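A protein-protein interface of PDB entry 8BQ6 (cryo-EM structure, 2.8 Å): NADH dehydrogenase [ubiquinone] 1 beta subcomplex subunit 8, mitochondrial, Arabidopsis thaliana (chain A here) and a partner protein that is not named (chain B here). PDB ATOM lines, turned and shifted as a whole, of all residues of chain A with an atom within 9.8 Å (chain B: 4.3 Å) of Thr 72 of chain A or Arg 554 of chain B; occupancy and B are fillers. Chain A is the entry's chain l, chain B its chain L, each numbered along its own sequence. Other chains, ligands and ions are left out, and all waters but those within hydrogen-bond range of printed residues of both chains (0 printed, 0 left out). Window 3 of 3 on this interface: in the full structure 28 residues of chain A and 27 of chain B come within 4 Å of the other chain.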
ATOM      1  N   ALA A  70      10.202  -4.345  25.623  1.00  0.00           N
ATOM      2  CA  ALA A  70       9.602  -3.323  26.473  1.00  0.00           C
ATOM      3  C   ALA A  70       9.266  -2.085  25.652  1.00  0.00           C
ATOM      4  O   ALA A  70       9.282  -0.963  26.161  1.00  0.00           O
ATOM      5  CB  ALA A  70      10.538  -2.969  27.621  1.00  0.00           C
ATOM      6  N   ASP A  71       8.959  -2.301  24.374  1.00  0.00           N
ATOM      7  CA  ASP A  71       8.702  -1.206  23.449  1.00  0.00           C
ATOM      8  C   ASP A  71       7.334  -1.344  22.797  1.00  0.00           C
ATOM      9  O   ASP A  71       6.631  -0.348  22.594  1.00  0.00           O
ATOM     10  CB  ASP A  71       9.798  -1.150  22.381  1.00  0.00           C
ATOM     11  CG  ASP A  71       9.399  -0.321  21.173  1.00  0.00           C
ATOM     12  OD1 ASP A  71       8.971   0.836  21.358  1.00  0.00           O
ATOM     13  OD2 ASP A  71       9.537  -0.815  20.033  1.00  0.00           O
ATOM     14  N   THR A  72       6.945  -2.580  22.476  1.00  0.00           N
ATOM     15  CA  THR A  72       5.729  -2.848  21.721  1.00  0.00           C
ATOM     16  C   THR A  72       4.528  -3.222  22.576  1.00  0.00           C
ATOM     17  O   THR A  72       3.396  -3.087  22.102  1.00  0.00           O
ATOM     18  CB  THR A  72       5.963  -3.984  20.716  1.00  0.00           C
ATOM     19  OG1 THR A  72       6.177  -5.209  21.428  1.00  0.00           O
ATOM     20  CG2 THR A  72       7.172  -3.696  19.835  1.00  0.00           C
ATOM     21  N   VAL A  73       4.733  -3.703  23.796  1.00  0.00           N
ATOM     22  CA  VAL A  73       3.635  -4.150  24.648  1.00  0.00           C
ATOM     23  C   VAL A  73       3.521  -3.221  25.847  1.00  0.00           C
ATOM     24  O   VAL A  73       4.522  -2.903  26.503  1.00  0.00           O
ATOM     25  CB  VAL A  73       3.824  -5.615  25.084  1.00  0.00           C
ATOM     26  CG1 VAL A  73       5.243  -5.852  25.574  1.00  0.00           C
ATOM     27  CG2 VAL A  73       2.811  -5.982  26.156  1.00  0.00           C
ATOM     28  N   GLY A  74       2.297  -2.789  26.137  1.00  0.00           N
ATOM     29  CA  GLY A  74       2.065  -1.798  27.166  1.00  0.00           C
ATOM     30  C   GLY A  74       2.376  -2.301  28.564  1.00  0.00           C
ATOM     31  O   GLY A  74       2.670  -3.473  28.801  1.00  0.00           O
ATOM     32  N   LYS A  75       2.306  -1.370  29.515  1.00  0.00           N
ATOM     33  CA  LYS A  75       2.687  -1.676  30.889  1.00  0.00           C
ATOM     34  C   LYS A  75       1.679  -2.610  31.550  1.00  0.00           C
ATOM     35  O   LYS A  75       2.034  -3.700  32.012  1.00  0.00           O
ATOM     36  CB  LYS A  75       2.834  -0.378  31.683  1.00  0.00           C
ATOM     37  CG  LYS A  75       3.302  -0.557  33.113  1.00  0.00           C
ATOM     38  CD  LYS A  75       2.454   0.283  34.041  1.00  0.00           C
ATOM     39  CE  LYS A  75       2.999   0.291  35.452  1.00  0.00           C
ATOM     40  NZ  LYS A  75       3.666   1.577  35.780  1.00  0.00           N
ATOM     41  N   GLU A  77      -0.792  -4.173  30.135  1.00  0.00           N
ATOM     42  CA  GLU A  77      -1.073  -5.325  29.284  1.00  0.00           C
ATOM     43  C   GLU A  77      -0.046  -6.428  29.507  1.00  0.00           C
ATOM     44  O   GLU A  77      -0.372  -7.620  29.457  1.00  0.00           O
ATOM     45  CB  GLU A  77      -1.097  -4.887  27.820  1.00  0.00           C
ATOM     46  CG  GLU A  77      -0.784  -5.976  26.814  1.00  0.00           C
ATOM     47  CD  GLU A  77      -1.399  -5.691  25.460  1.00  0.00           C
ATOM     48  OE1 GLU A  77      -0.982  -6.318  24.464  1.00  0.00           O
ATOM     49  OE2 GLU A  77      -2.303  -4.832  25.390  1.00  0.00           O
ATOM     50  N   ALA A  78       1.210  -6.043  29.739  1.00  0.00           N
ATOM     51  CA  ALA A  78       2.239  -7.015  30.095  1.00  0.00           C
ATOM     52  C   ALA A  78       1.949  -7.648  31.447  1.00  0.00           C
ATOM     53  O   ALA A  78       2.204  -8.840  31.654  1.00  0.00           O
ATOM     54  CB  ALA A  78       3.611  -6.343  30.105  1.00  0.00           C
ATOM     55  N   TRP A  81      -0.741 -10.289  30.857  1.00  0.00           N
ATOM     56  CA  TRP A  81      -0.252 -11.499  30.203  1.00  0.00           C
ATOM     57  C   TRP A  81       0.597 -12.329  31.154  1.00  0.00           C
ATOM     58  O   TRP A  81       0.496 -13.560  31.183  1.00  0.00           O
ATOM     59  CB  TRP A  81       0.543 -11.146  28.950  1.00  0.00           C
ATOM     60  CG  TRP A  81      -0.312 -10.952  27.759  1.00  0.00           C
ATOM     61  CD1 TRP A  81      -0.932  -9.803  27.383  1.00  0.00           C
ATOM     62  CD2 TRP A  81      -0.650 -11.934  26.775  1.00  0.00           C
ATOM     63  NE1 TRP A  81      -1.636 -10.002  26.225  1.00  0.00           N
ATOM     64  CE2 TRP A  81      -1.480 -11.304  25.830  1.00  0.00           C
ATOM     65  CE3 TRP A  81      -0.330 -13.283  26.600  1.00  0.00           C
ATOM     66  CZ2 TRP A  81      -1.995 -11.975  24.728  1.00  0.00           C
ATOM     67  CZ3 TRP A  81      -0.843 -13.947  25.505  1.00  0.00           C
ATOM     68  CH2 TRP A  81      -1.666 -13.293  24.584  1.00  0.00           C
ATOM     69  N   LEU A  82       1.455 -11.664  31.932  1.00  0.00           N
ATOM     70  CA  LEU A  82       2.271 -12.397  32.938  1.00  0.00           C
ATOM     71  C   LEU A  82       1.342 -12.979  34.008  1.00  0.00           C
ATOM     72  O   LEU A  82       1.593 -14.114  34.436  1.00  0.00           O
ATOM     73  CB  LEU A  82       3.315 -11.466  33.562  1.00  0.00           C
ATOM     74  CG  LEU A  82       4.132 -12.071  34.706  1.00  0.00           C
ATOM     75  CD1 LEU A  82       4.856 -13.333  34.265  1.00  0.00           C
ATOM     76  CD2 LEU A  82       5.118 -11.066  35.273  1.00  0.00           C
ATOM     77  N   THR B 550      -3.932 -10.563  15.906  1.00  0.00           N
ATOM     78  CA  THR B 550      -3.467  -9.817  17.073  1.00  0.00           C
ATOM     79  C   THR B 550      -3.147 -10.738  18.246  1.00  0.00           C
ATOM     80  O   THR B 550      -2.117 -10.564  18.908  1.00  0.00           O
ATOM     81  CB  THR B 550      -4.506  -8.765  17.476  1.00  0.00           C
ATOM     82  OG1 THR B 550      -3.854  -7.685  18.154  1.00  0.00           O
ATOM     83  CG2 THR B 550      -5.573  -9.344  18.392  1.00  0.00           C
ATOM     84  N   PHE B 551      -4.006 -11.721  18.524  1.00  0.00           N
ATOM     85  CA  PHE B 551      -3.744 -12.607  19.646  1.00  0.00           C
ATOM     86  C   PHE B 551      -2.516 -13.464  19.384  1.00  0.00           C
ATOM     87  O   PHE B 551      -1.710 -13.690  20.291  1.00  0.00           O
ATOM     88  CB  PHE B 551      -4.963 -13.478  19.940  1.00  0.00           C
ATOM     89  CG  PHE B 551      -4.818 -14.313  21.181  1.00  0.00           C
ATOM     90  CD1 PHE B 551      -5.386 -13.912  22.375  1.00  0.00           C
ATOM     91  CD2 PHE B 551      -4.120 -15.509  21.148  1.00  0.00           C
ATOM     92  CE1 PHE B 551      -5.247 -14.679  23.515  1.00  0.00           C
ATOM     93  CE2 PHE B 551      -3.980 -16.275  22.281  1.00  0.00           C
ATOM     94  CZ  PHE B 551      -4.546 -15.863  23.464  1.00  0.00           C
ATOM     95  N   CYS B 552      -2.361 -13.960  18.155  1.00  0.00           N
ATOM     96  CA  CYS B 552      -1.201 -14.792  17.853  1.00  0.00           C
ATOM     97  C   CYS B 552       0.081 -13.971  17.808  1.00  0.00           C
ATOM     98  O   CYS B 552       1.174 -14.511  18.005  1.00  0.00           O
ATOM     99  CB  CYS B 552      -1.402 -15.533  16.531  1.00  0.00           C
ATOM    100  SG  CYS B 552      -2.735 -16.746  16.536  1.00  0.00           S
ATOM    101  N   ASN B 553      -0.027 -12.670  17.523  1.00  0.00           N
ATOM    102  CA  ASN B 553       1.162 -11.825  17.509  1.00  0.00           C
ATOM    103  C   ASN B 553       1.632 -11.510  18.924  1.00  0.00           C
ATOM    104  O   ASN B 553       2.837 -11.538  19.206  1.00  0.00           O
ATOM    105  CB  ASN B 553       0.887 -10.542  16.728  1.00  0.00           C
ATOM    106  CG  ASN B 553       2.140  -9.733  16.484  1.00  0.00           C
ATOM    107  OD1 ASN B 553       2.427  -8.780  17.205  1.00  0.00           O
ATOM    108  ND2 ASN B 553       2.907 -10.121  15.473  1.00  0.00           N
ATOM    109  N   ARG B 554       0.697 -11.208  19.829  1.00  0.00           N
ATOM    110  CA  ARG B 554       1.055 -10.989  21.228  1.00  0.00           C
ATOM    111  C   ARG B 554       1.603 -12.262  21.854  1.00  0.00           C
ATOM    112  O   ARG B 554       2.497 -12.212  22.706  1.00  0.00           O
ATOM    113  CB  ARG B 554      -0.159 -10.499  22.017  1.00  0.00           C
ATOM    114  CG  ARG B 554      -0.653  -9.095  21.686  1.00  0.00           C
ATOM    115  CD  ARG B 554       0.424  -8.205  21.090  1.00  0.00           C
ATOM    116  NE  ARG B 554       0.172  -6.799  21.386  1.00  0.00           N
ATOM    117  CZ  ARG B 554       1.082  -5.838  21.313  1.00  0.00           C
ATOM    118  NH1 ARG B 554       2.332  -6.094  20.962  1.00  0.00           N
ATOM    119  NH2 ARG B 554       0.730  -4.588  21.599  1.00  0.00           N
ATOM    120  N   LEU B 555       1.062 -13.411  21.455  1.00  0.00           N
ATOM    121  CA  LEU B 555       1.546 -14.687  21.964  1.00  0.00           C
ATOM    122  C   LEU B 555       2.994 -14.933  21.556  1.00  0.00           C
ATOM    123  O   LEU B 555       3.790 -15.455  22.347  1.00  0.00           O
ATOM    124  CB  LEU B 555       0.638 -15.805  21.463  1.00  0.00           C
ATOM    125  CG  LEU B 555       0.561 -17.062  22.318  1.00  0.00           C
ATOM    126  CD1 LEU B 555      -0.744 -17.767  22.057  1.00  0.00           C
ATOM    127  CD2 LEU B 555       1.714 -17.967  21.976  1.00  0.00           C
ATOM    128  N   TYR B 556       3.348 -14.588  20.315  1.00  0.00           N
ATOM    129  CA  TYR B 556       4.734 -14.698  19.872  1.00  0.00           C
ATOM    130  C   TYR B 556       5.646 -13.819  20.712  1.00  0.00           C
ATOM    131  O   TYR B 556       6.755 -14.220  21.083  1.00  0.00           O
ATOM    132  CB  TYR B 556       4.850 -14.299  18.402  1.00  0.00           C
ATOM    133  CG  TYR B 556       6.110 -14.785  17.726  1.00  0.00           C
ATOM    134  CD1 TYR B 556       6.242 -16.105  17.330  1.00  0.00           C
ATOM    135  CD2 TYR B 556       7.183 -13.930  17.515  1.00  0.00           C
ATOM    136  CE1 TYR B 556       7.390 -16.552  16.714  1.00  0.00           C
ATOM    137  CE2 TYR B 556       8.340 -14.372  16.904  1.00  0.00           C
ATOM    138  CZ  TYR B 556       8.437 -15.685  16.507  1.00  0.00           C
ATOM    139  OH  TYR B 556       9.585 -16.133  15.896  1.00  0.00           O
ATOM    140  N   SER B 557       5.198 -12.599  21.000  1.00  0.00           N
ATOM    141  CA  SER B 557       6.009 -11.682  21.789  1.00  0.00           C
ATOM    142  C   SER B 557       6.014 -12.084  23.258  1.00  0.00           C
ATOM    143  O   SER B 557       6.972 -11.806  23.986  1.00  0.00           O
ATOM    144  CB  SER B 557       5.498 -10.253  21.606  1.00  0.00           C
ATOM    145  OG  SER B 557       4.576  -9.905  22.622  1.00  0.00           O
ATOM    146  N   PHE B 558       4.953 -12.755  23.709  1.00  0.00           N
ATOM    147  CA  PHE B 558       4.901 -13.206  25.096  1.00  0.00           C
ATOM    148  C   PHE B 558       6.016 -14.201  25.400  1.00  0.00           C
ATOM    149  O   PHE B 558       6.709 -14.084  26.415  1.00  0.00           O
ATOM    150  CB  PHE B 558       3.532 -13.817  25.393  1.00  0.00           C
ATOM    151  CG  PHE B 558       3.423 -14.408  26.763  1.00  0.00           C
ATOM    152  CD1 PHE B 558       3.199 -13.600  27.862  1.00  0.00           C
ATOM    153  CD2 PHE B 558       3.546 -15.773  26.954  1.00  0.00           C
ATOM    154  CE1 PHE B 558       3.103 -14.140  29.124  1.00  0.00           C
ATOM    155  CE2 PHE B 558       3.452 -16.317  28.215  1.00  0.00           C
ATOM    156  CZ  PHE B 558       3.228 -15.500  29.300  1.00  0.00           C
ATOM    157  N   LYS B 561       9.623 -12.449  24.688  1.00  0.00           N
ATOM    158  CA  LYS B 561      10.056 -11.469  25.722  1.00  0.00           C
ATOM    159  C   LYS B 561       9.976 -12.086  27.122  1.00  0.00           C
ATOM    160  O   LYS B 561       9.808 -11.307  28.077  1.00  0.00           O
ATOM    161  CB  LYS B 561       9.242 -10.176  25.605  1.00  0.00           C
ATOM    162  CG  LYS B 561       9.471  -9.396  24.317  1.00  0.00           C
ATOM    163  CD  LYS B 561       8.675  -8.113  24.232  1.00  0.00           C
ATOM    164  CE  LYS B 561       9.137  -7.216  23.104  1.00  0.00           C
ATOM    165  NZ  LYS B 561       8.396  -5.934  23.078  1.00  0.00           N
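The guanidinium group of Arg 554 of chain B lies within hydrogen-bond range of the backbone carbonyl oxygen of Thr 72 of chain A, 3.1 Å away.
The guanidinium group of Arg 554 of chain B lies within salt-bridge range of the side-chain carboxylate of Glu 77 of chain A.
The side-chain amino group of Lys 561 of chain B lies within hydrogen-bond range of the side-chain hydroxyl of Thr 72 of chain A (2.9 Å).
OG of Ser 557 of chain B lies within hydrogen-bond range of O of Arg 554 of chain B (3.1 Å).
Among the printed residues, pairs that only touch across the chains: Trp 81 of chain A with Phe 558 of chain B (3.4 Å), Ala 70 of chain A with Lys 561 of chain B (3.5 Å), Trp 81 of chain A with Arg 554 of chain B (3.6 Å), Asp 71 of chain A with Lys 561 of chain B (3.9 Å) and Trp 81 of chain A with Phe 551 of chain B (3.99 Å).
Printed residues of chain B within 4 Å of Asp 71 of chain A: Lys 561 (3.9 Å).
Of the printed residues of chain B, Thr 72 of chain A touches Arg 554 (3.1 Å) and Lys 561 (2.9 Å).
Of the printed residues of chain B, Trp 81 of chain A touches Phe 551 (3.99 Å), Arg 554 (3.6 Å) and Phe 558 (3.4 Å).
Printed residues of chain A within 4 Å of Phe 551 of chain B: Trp 81 (3.99 Å).
No residue of chain A comes within 4 Å of Asn 553 of chain B.
Arg 554 of chain B touches three residues of chain A.
No residue of chain A comes within 4 Å of Ser 557 of chain B.
Of the printed residues of chain A, Phe 558 of chain B touches Trp 81 (3.4 Å).
The nearest printed residue of chain B that does not touch Thr 72 of chain A is Ser 557 of chain B (5.1 Å).
Among the printed residues, Asp or Glu carboxylates within 4 Å of a Lys or Arg side-chain nitrogen of the other chain: Glu 77 of chain A with Arg 554 of chain B.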
